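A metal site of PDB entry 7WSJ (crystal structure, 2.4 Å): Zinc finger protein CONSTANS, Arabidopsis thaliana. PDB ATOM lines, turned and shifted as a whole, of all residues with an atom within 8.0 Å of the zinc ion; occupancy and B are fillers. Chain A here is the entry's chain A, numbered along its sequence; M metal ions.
SG of Cys 76 lies close to N of Ala 78. O of Ala 81 lies within hydrogen-bond range of N of Cys 76 (2.9 Å). The guanidinium group (NE) of Arg 103 lies within hydrogen-bond range of a ring nitrogen (ND1) of His 92, at 3.4 Å. A ring nitrogen (ND1) of His 92 is in hydrogen-bond range of the backbone carbonyl oxygen (O) of Asp 88, 2.7 Å away. The guanidinium group of Arg 103 is in hydrogen-bond range of the backbone carbonyl oxygen of His 101 (3.2 Å).
Four residues have an atom within 4 Å of the zinc ion: Cys 76, Asp 79, His 92 and His 101.
The side-chain carboxylate (OD2) of Asp 79 is bound to the zinc ion (2.0 Å). The zinc ion is bound by SG of Cys 76, 2.3 Å away. A ring nitrogen (NE2) of His 92 binds the zinc ion (2.3 Å). ND1 of His 101 is bound to the zinc ion. The zinc ion has four donor atoms within binding distance.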
ATOM      1  N   LEU A  75       6.785 -21.989   7.681  1.00  0.00           N
ATOM      2  CA  LEU A  75       7.566 -23.064   7.088  1.00  0.00           C
ATOM      3  C   LEU A  75       8.982 -22.556   6.820  1.00  0.00           C
ATOM      4  O   LEU A  75       9.156 -21.492   6.211  1.00  0.00           O
ATOM      5  CB  LEU A  75       6.927 -23.544   5.789  1.00  0.00           C
ATOM      6  CG  LEU A  75       7.767 -24.506   4.935  1.00  0.00           C
ATOM      7  CD1 LEU A  75       7.870 -25.874   5.596  1.00  0.00           C
ATOM      8  CD2 LEU A  75       7.196 -24.616   3.538  1.00  0.00           C
ATOM      9  N   CYS A  76       9.967 -23.314   7.275  1.00  0.00           N
ATOM     10  CA  CYS A  76      11.372 -23.022   7.035  1.00  0.00           C
ATOM     11  C   CYS A  76      11.960 -24.203   6.270  1.00  0.00           C
ATOM     12  O   CYS A  76      12.058 -25.318   6.808  1.00  0.00           O
ATOM     13  CB  CYS A  76      12.128 -22.780   8.343  1.00  0.00           C
ATOM     14  SG  CYS A  76      13.878 -22.427   8.096  1.00  0.00           S
ATOM     15  N   GLU A  77      12.348 -23.957   5.012  1.00  0.00           N
ATOM     16  CA  GLU A  77      12.919 -24.999   4.185  1.00  0.00           C
ATOM     17  C   GLU A  77      14.319 -25.386   4.645  1.00  0.00           C
ATOM     18  O   GLU A  77      14.707 -26.562   4.548  1.00  0.00           O
ATOM     19  CB  GLU A  77      12.947 -24.554   2.720  1.00  0.00           C
ATOM     20  CG  GLU A  77      11.571 -24.426   2.089  1.00  0.00           C
ATOM     21  CD  GLU A  77      11.563 -23.538   0.852  1.00  0.00           C
ATOM     22  OE1 GLU A  77      10.705 -22.637   0.768  1.00  0.00           O
ATOM     23  OE2 GLU A  77      12.428 -23.741  -0.028  1.00  0.00           O
ATOM     24  N   ALA A  78      15.097 -24.419   5.149  1.00  0.00           N
ATOM     25  CA  ALA A  78      16.434 -24.742   5.632  1.00  0.00           C
ATOM     26  C   ALA A  78      16.368 -25.707   6.809  1.00  0.00           C
ATOM     27  O   ALA A  78      17.066 -26.727   6.840  1.00  0.00           O
ATOM     28  CB  ALA A  78      17.179 -23.461   6.015  1.00  0.00           C
ATOM     29  N   ASP A  79      15.527 -25.390   7.792  1.00  0.00           N
ATOM     30  CA  ASP A  79      15.295 -26.312   8.904  1.00  0.00           C
ATOM     31  C   ASP A  79      14.410 -27.486   8.528  1.00  0.00           C
ATOM     32  O   ASP A  79      14.302 -28.425   9.328  1.00  0.00           O
ATOM     33  CB  ASP A  79      14.671 -25.561  10.087  1.00  0.00           C
ATOM     34  CG  ASP A  79      15.654 -24.665  10.793  1.00  0.00           C
ATOM     35  OD1 ASP A  79      16.851 -25.001  10.821  1.00  0.00           O
ATOM     36  OD2 ASP A  79      15.236 -23.612  11.326  1.00  0.00           O
ATOM     37  N   ASP A  80      13.773 -27.456   7.364  1.00  0.00           N
ATOM     38  CA  ASP A  80      12.805 -28.470   6.952  1.00  0.00           C
ATOM     39  C   ASP A  80      11.768 -28.681   8.049  1.00  0.00           C
ATOM     40  O   ASP A  80      11.547 -29.787   8.541  1.00  0.00           O
ATOM     41  CB  ASP A  80      13.517 -29.783   6.580  1.00  0.00           C
ATOM     42  CG  ASP A  80      12.564 -30.827   6.014  1.00  0.00           C
ATOM     43  OD1 ASP A  80      11.784 -30.476   5.103  1.00  0.00           O
ATOM     44  OD2 ASP A  80      12.604 -31.979   6.477  1.00  0.00           O
ATOM     45  N   ALA A  81      11.121 -27.587   8.430  1.00  0.00           N
ATOM     46  CA  ALA A  81      10.278 -27.621   9.626  1.00  0.00           C
ATOM     47  C   ALA A  81       9.135 -26.627   9.509  1.00  0.00           C
ATOM     48  O   ALA A  81       9.313 -25.510   9.027  1.00  0.00           O
ATOM     49  CB  ALA A  81      11.099 -27.331  10.886  1.00  0.00           C
ATOM     50  N   LEU A  83       6.699 -24.642  11.986  1.00  0.00           N
ATOM     51  CA  LEU A  83       6.739 -24.271  13.392  1.00  0.00           C
ATOM     52  C   LEU A  83       5.633 -23.276  13.729  1.00  0.00           C
ATOM     53  O   LEU A  83       5.187 -22.501  12.871  1.00  0.00           O
ATOM     54  CB  LEU A  83       8.096 -23.652  13.747  1.00  0.00           C
ATOM     55  CG  LEU A  83       9.306 -24.522  13.399  1.00  0.00           C
ATOM     56  CD1 LEU A  83      10.608 -23.756  13.594  1.00  0.00           C
ATOM     57  CD2 LEU A  83       9.302 -25.787  14.236  1.00  0.00           C
ATOM     58  N   ASP A  88       9.077 -20.721  16.107  1.00  0.00           N
ATOM     59  CA  ASP A  88       9.781 -20.037  15.027  1.00  0.00           C
ATOM     60  C   ASP A  88      10.726 -18.979  15.590  1.00  0.00           C
ATOM     61  O   ASP A  88      11.923 -18.950  15.243  1.00  0.00           O
ATOM     62  CB  ASP A  88       8.771 -19.414  14.077  1.00  0.00           C
ATOM     63  CG  ASP A  88       9.424 -18.697  12.916  1.00  0.00           C
ATOM     64  OD1 ASP A  88      10.159 -19.348  12.157  1.00  0.00           O
ATOM     65  OD2 ASP A  88       9.188 -17.478  12.773  1.00  0.00           O
ATOM     66  N   VAL A  91      13.653 -20.558  17.612  1.00  0.00           N
ATOM     67  CA  VAL A  91      14.646 -21.211  16.766  1.00  0.00           C
ATOM     68  C   VAL A  91      15.502 -20.180  16.049  1.00  0.00           C
ATOM     69  O   VAL A  91      16.733 -20.292  15.995  1.00  0.00           O
ATOM     70  CB  VAL A  91      13.961 -22.172  15.786  1.00  0.00           C
ATOM     71  CG1 VAL A  91      14.921 -22.561  14.671  1.00  0.00           C
ATOM     72  CG2 VAL A  91      13.469 -23.411  16.515  1.00  0.00           C
ATOM     73  N   HIS A  92      14.870 -19.149  15.485  1.00  0.00           N
ATOM     74  CA  HIS A  92      15.563 -18.226  14.603  1.00  0.00           C
ATOM     75  C   HIS A  92      16.075 -16.976  15.307  1.00  0.00           C
ATOM     76  O   HIS A  92      16.521 -16.040  14.644  1.00  0.00           O
ATOM     77  CB  HIS A  92      14.649 -17.836  13.444  1.00  0.00           C
ATOM     78  CG  HIS A  92      14.177 -19.000  12.637  1.00  0.00           C
ATOM     79  ND1 HIS A  92      13.023 -19.686  12.927  1.00  0.00           N
ATOM     80  CD2 HIS A  92      14.720 -19.619  11.568  1.00  0.00           C
ATOM     81  CE1 HIS A  92      12.866 -20.669  12.057  1.00  0.00           C
ATOM     82  NE2 HIS A  92      13.880 -20.646  11.223  1.00  0.00           N
ATOM     83  N   LEU A  97      23.186 -16.924  12.578  1.00  0.00           N
ATOM     84  CA  LEU A  97      23.070 -17.861  11.464  1.00  0.00           C
ATOM     85  C   LEU A  97      21.631 -18.329  11.278  1.00  0.00           C
ATOM     86  O   LEU A  97      21.159 -18.474  10.148  1.00  0.00           O
ATOM     87  CB  LEU A  97      24.011 -19.042  11.686  1.00  0.00           C
ATOM     88  CG  LEU A  97      24.511 -19.786  10.459  1.00  0.00           C
ATOM     89  CD1 LEU A  97      25.112 -18.815   9.456  1.00  0.00           C
ATOM     90  CD2 LEU A  97      25.547 -20.821  10.884  1.00  0.00           C
ATOM     91  N   ALA A  98      20.920 -18.561  12.387  1.00  0.00           N
ATOM     92  CA  ALA A  98      19.507 -18.931  12.291  1.00  0.00           C
ATOM     93  C   ALA A  98      18.643 -17.753  11.876  1.00  0.00           C
ATOM     94  O   ALA A  98      17.627 -17.945  11.202  1.00  0.00           O
ATOM     95  CB  ALA A  98      19.029 -19.505  13.622  1.00  0.00           C
ATOM     96  N   ARG A  99      19.038 -16.529  12.242  1.00  0.00           N
ATOM     97  CA  ARG A  99      18.256 -15.361  11.869  1.00  0.00           C
ATOM     98  C   ARG A  99      18.184 -15.190  10.360  1.00  0.00           C
ATOM     99  O   ARG A  99      17.222 -14.611   9.841  1.00  0.00           O
ATOM    100  CB  ARG A  99      18.848 -14.095  12.503  1.00  0.00           C
ATOM    101  CG  ARG A  99      18.778 -14.069  14.016  1.00  0.00           C
ATOM    102  CD  ARG A  99      19.017 -12.665  14.568  1.00  0.00           C
ATOM    103  NE  ARG A  99      18.327 -12.457  15.839  1.00  0.00           N
ATOM    104  CZ  ARG A  99      17.101 -11.943  15.938  1.00  0.00           C
ATOM    105  NH1 ARG A  99      16.446 -11.568  14.855  1.00  0.00           N
ATOM    106  NH2 ARG A  99      16.548 -11.788  17.136  1.00  0.00           N
ATOM    107  N   ARG A 100      19.178 -15.704   9.631  1.00  0.00           N
ATOM    108  CA  ARG A 100      19.217 -15.523   8.175  1.00  0.00           C
ATOM    109  C   ARG A 100      18.178 -16.366   7.458  1.00  0.00           C
ATOM    110  O   ARG A 100      17.866 -16.078   6.296  1.00  0.00           O
ATOM    111  CB  ARG A 100      20.610 -15.849   7.642  1.00  0.00           C
ATOM    112  CG  ARG A 100      21.704 -14.922   8.151  1.00  0.00           C
ATOM    113  CD  ARG A 100      22.861 -14.804   7.172  1.00  0.00           C
ATOM    114  NE  ARG A 100      23.667 -16.022   7.082  1.00  0.00           N
ATOM    115  CZ  ARG A 100      23.599 -16.895   6.088  1.00  0.00           C
ATOM    116  NH1 ARG A 100      22.760 -16.705   5.078  1.00  0.00           N
ATOM    117  NH2 ARG A 100      24.381 -17.974   6.094  1.00  0.00           N
ATOM    118  N   HIS A 101      17.647 -17.402   8.105  1.00  0.00           N
ATOM    119  CA  HIS A 101      16.703 -18.297   7.452  1.00  0.00           C
ATOM    120  C   HIS A 101      15.467 -17.549   6.968  1.00  0.00           C
ATOM    121  O   HIS A 101      14.890 -16.749   7.711  1.00  0.00           O
ATOM    122  CB  HIS A 101      16.288 -19.416   8.412  1.00  0.00           C
ATOM    123  CG  HIS A 101      17.410 -20.319   8.813  1.00  0.00           C
ATOM    124  ND1 HIS A 101      17.277 -21.281   9.799  1.00  0.00           N
ATOM    125  CD2 HIS A 101      18.675 -20.419   8.364  1.00  0.00           C
ATOM    126  CE1 HIS A 101      18.417 -21.931   9.936  1.00  0.00           C
ATOM    127  NE2 HIS A 101      19.284 -21.428   9.074  1.00  0.00           N
ATOM    128  N   GLN A 102      15.077 -17.796   5.723  1.00  0.00           N
ATOM    129  CA  GLN A 102      13.856 -17.233   5.168  1.00  0.00           C
ATOM    130  C   GLN A 102      12.706 -18.210   5.403  1.00  0.00           C
ATOM    131  O   GLN A 102      12.799 -19.384   5.034  1.00  0.00           O
ATOM    132  CB  GLN A 102      14.004 -16.944   3.675  1.00  0.00           C
ATOM    133  CG  GLN A 102      15.175 -16.044   3.329  1.00  0.00           C
ATOM    134  CD  GLN A 102      15.239 -15.725   1.850  1.00  0.00           C
ATOM    135  OE1 GLN A 102      16.310 -15.692   1.254  1.00  0.00           O
ATOM    136  NE2 GLN A 102      14.081 -15.485   1.243  1.00  0.00           N
ATOM    137  N   ARG A 103      11.634 -17.727   6.016  1.00  0.00           N
ATOM    138  CA  ARG A 103      10.469 -18.548   6.311  1.00  0.00           C
ATOM    139  C   ARG A 103       9.255 -17.985   5.597  1.00  0.00           C
ATOM    140  O   ARG A 103       9.155 -16.773   5.355  1.00  0.00           O
ATOM    141  CB  ARG A 103      10.197 -18.625   7.825  1.00  0.00           C
ATOM    142  CG  ARG A 103      11.304 -19.299   8.614  1.00  0.00           C
ATOM    143  CD  ARG A 103      12.287 -18.288   9.176  1.00  0.00           C
ATOM    144  NE  ARG A 103      11.820 -17.708  10.435  1.00  0.00           N
ATOM    145  CZ  ARG A 103      12.408 -16.692  11.059  1.00  0.00           C
ATOM    146  NH1 ARG A 103      13.488 -16.120  10.530  1.00  0.00           N
ATOM    147  NH2 ARG A 103      11.918 -16.241  12.203  1.00  0.00           N
HETATM  148 ZN    ZN M   1      15.135 -22.132   9.996  1.00  0.00          ZN
